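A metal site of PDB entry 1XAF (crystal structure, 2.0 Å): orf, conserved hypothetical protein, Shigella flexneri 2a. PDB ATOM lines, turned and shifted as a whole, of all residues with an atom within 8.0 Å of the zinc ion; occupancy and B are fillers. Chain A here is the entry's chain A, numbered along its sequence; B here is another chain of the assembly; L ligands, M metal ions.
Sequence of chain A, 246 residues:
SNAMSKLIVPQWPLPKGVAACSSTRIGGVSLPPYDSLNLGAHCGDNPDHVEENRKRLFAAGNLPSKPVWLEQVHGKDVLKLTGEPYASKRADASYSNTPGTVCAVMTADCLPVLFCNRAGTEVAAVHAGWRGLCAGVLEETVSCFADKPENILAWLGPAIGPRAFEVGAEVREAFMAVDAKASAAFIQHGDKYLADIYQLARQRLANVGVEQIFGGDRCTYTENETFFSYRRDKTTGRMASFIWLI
The zinc ion is bound by an oxygen (O2) of the ligand, at 2.0 Å.
The zinc ion is bound by NE2 of His 127 (2.1 Å).
SG of Cys 110 binds the zinc ion (2.1 Å).
The zinc ion is bound by a ring nitrogen (NE2) of His 74, 2.2 Å away.
The zinc ion has four donor atoms within binding distance.
A ring nitrogen (ND1) of His 127 sits at hydrogen-bond distance from the side-chain carboxylate of Asp 92 (2.6 Å).
The side-chain carboxylate (OD1) of Asp 92 sits at hydrogen-bond distance from the backbone NH (N) of His 74, 2.8 Å away.
Three residues have an atom within 4 Å of the zinc ion: His 74, Cys 110 and His 127.
Along chain A the residues within 4 Å of the zinc ion span positions 74 to 127.
The nearest printed residue that does not touch the zinc ion is Gly 129 (4.8 Å).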
ATOM      1  N   GLN A  72     -16.972  -7.766  -2.325  1.00  0.00           N
ATOM      2  CA  GLN A  72     -17.497  -8.271  -1.044  1.00  0.00           C
ATOM      3  C   GLN A  72     -17.947  -7.132  -0.152  1.00  0.00           C
ATOM      4  O   GLN A  72     -17.174  -6.209   0.103  1.00  0.00           O
ATOM      5  CB  GLN A  72     -16.433  -9.099  -0.300  1.00  0.00           C
ATOM      6  CG  GLN A  72     -15.991 -10.338  -1.084  1.00  0.00           C
ATOM      7  CD  GLN A  72     -14.735 -11.006  -0.521  1.00  0.00           C
ATOM      8  OE1 GLN A  72     -14.218 -10.641   0.552  1.00  0.00           O
ATOM      9  NE2 GLN A  72     -14.244 -11.966  -1.242  1.00  0.00           N
ATOM     10  N   VAL A  73     -19.163  -7.233   0.359  1.00  0.00           N
ATOM     11  CA  VAL A  73     -19.766  -6.117   1.130  1.00  0.00           C
ATOM     12  C   VAL A  73     -20.153  -6.567   2.570  1.00  0.00           C
ATOM     13  O   VAL A  73     -20.861  -5.846   3.290  1.00  0.00           O
ATOM     14  CB  VAL A  73     -20.966  -5.495   0.345  1.00  0.00           C
ATOM     15  CG1 VAL A  73     -20.501  -4.755  -0.891  1.00  0.00           C
ATOM     16  CG2 VAL A  73     -21.967  -6.539  -0.057  1.00  0.00           C
ATOM     17  N   HIS A  74     -19.686  -7.752   2.969  1.00  0.00           N
ATOM     18  CA  HIS A  74     -20.012  -8.317   4.290  1.00  0.00           C
ATOM     19  C   HIS A  74     -21.491  -8.607   4.476  1.00  0.00           C
ATOM     20  O   HIS A  74     -21.985  -8.600   5.604  1.00  0.00           O
ATOM     21  CB  HIS A  74     -19.451  -7.453   5.433  1.00  0.00           C
ATOM     22  CG  HIS A  74     -17.973  -7.584   5.589  1.00  0.00           C
ATOM     23  ND1 HIS A  74     -17.082  -6.925   4.780  1.00  0.00           N
ATOM     24  CD2 HIS A  74     -17.219  -8.352   6.415  1.00  0.00           C
ATOM     25  CE1 HIS A  74     -15.844  -7.239   5.121  1.00  0.00           C
ATOM     26  NE2 HIS A  74     -15.896  -8.092   6.123  1.00  0.00           N
ATOM     27  N   ASP A  92     -21.082 -11.965  -1.252  1.00  0.00           N
ATOM     28  CA  ASP A  92     -20.061 -12.460  -0.329  1.00  0.00           C
ATOM     29  C   ASP A  92     -19.847 -13.960  -0.460  1.00  0.00           C
ATOM     30  O   ASP A  92     -19.094 -14.533   0.319  1.00  0.00           O
ATOM     31  CB  ASP A  92     -20.351 -12.017   1.092  1.00  0.00           C
ATOM     32  CG  ASP A  92     -20.042 -10.518   1.322  1.00  0.00           C
ATOM     33  OD1 ASP A  92     -18.908 -10.198   1.790  1.00  0.00           O
ATOM     34  OD2 ASP A  92     -20.927  -9.666   1.025  1.00  0.00           O
ATOM     35  N   MET A 106     -11.807 -13.427  -0.541  1.00  0.00           N
ATOM     36  CA  MET A 106     -10.675 -12.680  -0.039  1.00  0.00           C
ATOM     37  C   MET A 106     -10.921 -12.341   1.430  1.00  0.00           C
ATOM     38  O   MET A 106     -11.968 -11.813   1.765  1.00  0.00           O
ATOM     39  CB  MET A 106     -10.566 -11.396  -0.880  1.00  0.00           C
ATOM     40  CG  MET A 106      -9.843 -10.257  -0.232  1.00  0.00           C
ATOM     41  SD  MET A 106      -8.801  -9.441  -1.595  1.00  0.00           S
ATOM     42  CE  MET A 106      -7.721 -11.132  -1.864  1.00  0.00           C
ATOM     43  N   THR A 107      -9.966 -12.647   2.308  1.00  0.00           N
ATOM     44  CA  THR A 107     -10.196 -12.561   3.757  1.00  0.00           C
ATOM     45  C   THR A 107      -8.893 -12.159   4.455  1.00  0.00           C
ATOM     46  O   THR A 107      -7.815 -12.299   3.888  1.00  0.00           O
ATOM     47  CB  THR A 107     -10.663 -13.933   4.382  1.00  0.00           C
ATOM     48  OG1 THR A 107      -9.586 -14.876   4.331  1.00  0.00           O
ATOM     49  CG2 THR A 107     -11.916 -14.511   3.682  1.00  0.00           C
ATOM     50  N   ALA A 108      -9.017 -11.656   5.680  1.00  0.00           N
ATOM     51  CA  ALA A 108      -7.871 -11.502   6.620  1.00  0.00           C
ATOM     52  C   ALA A 108      -8.433 -11.384   8.023  1.00  0.00           C
ATOM     53  O   ALA A 108      -8.241 -10.368   8.695  1.00  0.00           O
ATOM     54  CB  ALA A 108      -7.014 -10.286   6.259  1.00  0.00           C
ATOM     55  N   ASP A 109      -9.178 -12.423   8.404  1.00  0.00           N
ATOM     56  CA  ASP A 109      -9.860 -12.617   9.703  1.00  0.00           C
ATOM     57  C   ASP A 109     -11.264 -13.234   9.545  1.00  0.00           C
ATOM     58  O   ASP A 109     -11.638 -14.098  10.351  1.00  0.00           O
ATOM     59  CB  ASP A 109     -10.057 -11.329  10.502  1.00  0.00           C
ATOM     60  CG  ASP A 109      -8.869 -10.958  11.377  1.00  0.00           C
ATOM     61  OD1 ASP A 109      -7.882 -11.713  11.550  1.00  0.00           O
ATOM     62  OD2 ASP A 109      -8.968  -9.862  11.933  1.00  0.00           O
ATOM     63  N   CYS A 110     -12.049 -12.767   8.541  1.00  0.00           N
ATOM     64  CA  CYS A 110     -13.347 -13.399   8.293  1.00  0.00           C
ATOM     65  C   CYS A 110     -13.206 -14.855   7.895  1.00  0.00           C
ATOM     66  O   CYS A 110     -12.184 -15.281   7.374  1.00  0.00           O
ATOM     67  CB  CYS A 110     -14.206 -12.636   7.295  1.00  0.00           C
ATOM     68  SG  CYS A 110     -14.572 -10.917   7.822  1.00  0.00           S
ATOM     69  N   LEU A 111     -14.225 -15.622   8.188  1.00  0.00           N
ATOM     70  CA  LEU A 111     -14.218 -17.027   7.900  1.00  0.00           C
ATOM     71  C   LEU A 111     -14.385 -17.296   6.417  1.00  0.00           C
ATOM     72  O   LEU A 111     -15.409 -16.897   5.838  1.00  0.00           O
ATOM     73  CB  LEU A 111     -15.383 -17.672   8.660  1.00  0.00           C
ATOM     74  CG  LEU A 111     -15.604 -19.156   8.402  1.00  0.00           C
ATOM     75  CD1 LEU A 111     -14.400 -19.871   8.900  1.00  0.00           C
ATOM     76  CD2 LEU A 111     -16.875 -19.622   9.211  1.00  0.00           C
ATOM     77  N   HIS A 127     -17.268 -15.837   1.878  1.00  0.00           N
ATOM     78  CA  HIS A 127     -16.631 -14.919   2.800  1.00  0.00           C
ATOM     79  C   HIS A 127     -17.636 -14.633   3.946  1.00  0.00           C
ATOM     80  O   HIS A 127     -18.585 -13.889   3.810  1.00  0.00           O
ATOM     81  CB  HIS A 127     -16.144 -13.639   2.081  1.00  0.00           C
ATOM     82  CG  HIS A 127     -15.961 -12.433   2.967  1.00  0.00           C
ATOM     83  ND1 HIS A 127     -16.798 -11.335   2.908  1.00  0.00           N
ATOM     84  CD2 HIS A 127     -15.043 -12.149   3.927  1.00  0.00           C
ATOM     85  CE1 HIS A 127     -16.410 -10.430   3.779  1.00  0.00           C
ATOM     86  NE2 HIS A 127     -15.346 -10.904   4.425  1.00  0.00           N
ATOM     87  N   ALA A 128     -17.424 -15.308   5.066  1.00  0.00           N
ATOM     88  CA  ALA A 128     -18.416 -15.224   6.124  1.00  0.00           C
ATOM     89  C   ALA A 128     -17.928 -14.344   7.267  1.00  0.00           C
ATOM     90  O   ALA A 128     -17.334 -14.842   8.220  1.00  0.00           O
ATOM     91  CB  ALA A 128     -18.787 -16.649   6.610  1.00  0.00           C
ATOM     92  N   GLY A 129     -18.127 -13.030   7.136  1.00  0.00           N
ATOM     93  CA  GLY A 129     -18.027 -12.119   8.270  1.00  0.00           C
ATOM     94  C   GLY A 129     -19.107 -12.464   9.278  1.00  0.00           C
ATOM     95  O   GLY A 129     -20.056 -13.175   8.932  1.00  0.00           O
ATOM     96  N   TRP A 130     -18.979 -11.997  10.514  1.00  0.00           N
ATOM     97  CA  TRP A 130     -20.011 -12.303  11.518  1.00  0.00           C
ATOM     98  C   TRP A 130     -21.429 -11.856  11.109  1.00  0.00           C
ATOM     99  O   TRP A 130     -22.395 -12.560  11.396  1.00  0.00           O
ATOM    100  CB  TRP A 130     -19.675 -11.752  12.907  1.00  0.00           C
ATOM    101  CG  TRP A 130     -19.899 -10.257  13.111  1.00  0.00           C
ATOM    102  CD1 TRP A 130     -18.970  -9.257  12.967  1.00  0.00           C
ATOM    103  CD2 TRP A 130     -21.115  -9.623  13.563  1.00  0.00           C
ATOM    104  NE1 TRP A 130     -19.545  -8.030  13.270  1.00  0.00           N
ATOM    105  CE2 TRP A 130     -20.854  -8.229  13.635  1.00  0.00           C
ATOM    106  CE3 TRP A 130     -22.410 -10.090  13.869  1.00  0.00           C
ATOM    107  CZ2 TRP A 130     -21.843  -7.293  14.039  1.00  0.00           C
ATOM    108  CZ3 TRP A 130     -23.388  -9.158  14.254  1.00  0.00           C
ATOM    109  CH2 TRP A 130     -23.092  -7.785  14.333  1.00  0.00           C
ATOM    110  N   TYR A 230      -6.587  -8.410   9.905  1.00  0.00           N
ATOM    111  CA  TYR A 230      -7.070  -7.027   9.975  1.00  0.00           C
ATOM    112  C   TYR A 230      -7.212  -6.480  11.407  1.00  0.00           C
ATOM    113  O   TYR A 230      -6.892  -5.320  11.693  1.00  0.00           O
ATOM    114  CB  TYR A 230      -8.396  -6.902   9.246  1.00  0.00           C
ATOM    115  CG  TYR A 230      -8.997  -5.519   9.234  1.00  0.00           C
ATOM    116  CD1 TYR A 230      -8.593  -4.553   8.312  1.00  0.00           C
ATOM    117  CD2 TYR A 230     -10.033  -5.190  10.110  1.00  0.00           C
ATOM    118  CE1 TYR A 230      -9.156  -3.301   8.305  1.00  0.00           C
ATOM    119  CE2 TYR A 230     -10.612  -3.929  10.118  1.00  0.00           C
ATOM    120  CZ  TYR A 230     -10.165  -2.989   9.208  1.00  0.00           C
ATOM    121  OH  TYR A 230     -10.754  -1.756   9.195  1.00  0.00           O
ATOM    122  N   ARG A 238      -4.023  -9.360   2.257  1.00  0.00           N
ATOM    123  CA  ARG A 238      -5.196 -10.232   2.229  1.00  0.00           C
ATOM    124  C   ARG A 238      -4.779 -11.562   1.674  1.00  0.00           C
ATOM    125  O   ARG A 238      -3.954 -11.593   0.754  1.00  0.00           O
ATOM    126  CB  ARG A 238      -6.301  -9.664   1.304  1.00  0.00           C
ATOM    127  CG  ARG A 238      -6.869  -8.335   1.759  1.00  0.00           C
ATOM    128  CD  ARG A 238      -7.714  -8.510   3.087  1.00  0.00           C
ATOM    129  NE  ARG A 238      -8.295  -7.227   3.509  1.00  0.00           N
ATOM    130  CZ  ARG A 238      -7.681  -6.236   4.145  1.00  0.00           C
ATOM    131  NH1 ARG A 238      -6.392  -6.313   4.493  1.00  0.00           N
ATOM    132  NH2 ARG A 238      -8.369  -5.142   4.460  1.00  0.00           N
ATOM    133  N   ASN B 224     -16.538  -1.114   8.608  1.00  0.00           N
ATOM    134  CA  ASN B 224     -17.944  -1.511   8.648  1.00  0.00           C
ATOM    135  C   ASN B 224     -18.516  -1.706  10.040  1.00  0.00           C
ATOM    136  O   ASN B 224     -19.729  -1.654  10.233  1.00  0.00           O
ATOM    137  CB  ASN B 224     -18.222  -2.686   7.702  1.00  0.00           C
ATOM    138  CG  ASN B 224     -17.293  -3.837   7.906  1.00  0.00           C
ATOM    139  OD1 ASN B 224     -17.345  -4.517   8.920  1.00  0.00           O
ATOM    140  ND2 ASN B 224     -16.435  -4.082   6.921  1.00  0.00           N
HETATM  141  C1  LIG L   1     -11.618  -9.408   5.974  1.00  0.00           C
HETATM  142  O1  LIG L   1     -11.489 -10.641   6.198  1.00  0.00           O
HETATM  143  O2  LIG L   1     -12.762  -8.963   5.605  1.00  0.00           O
HETATM  144  C2  LIG L   1     -10.451  -8.468   6.114  1.00  0.00           C
HETATM  145 ZN    ZN M   1     -14.529  -9.796   6.012  1.00  0.00          ZN
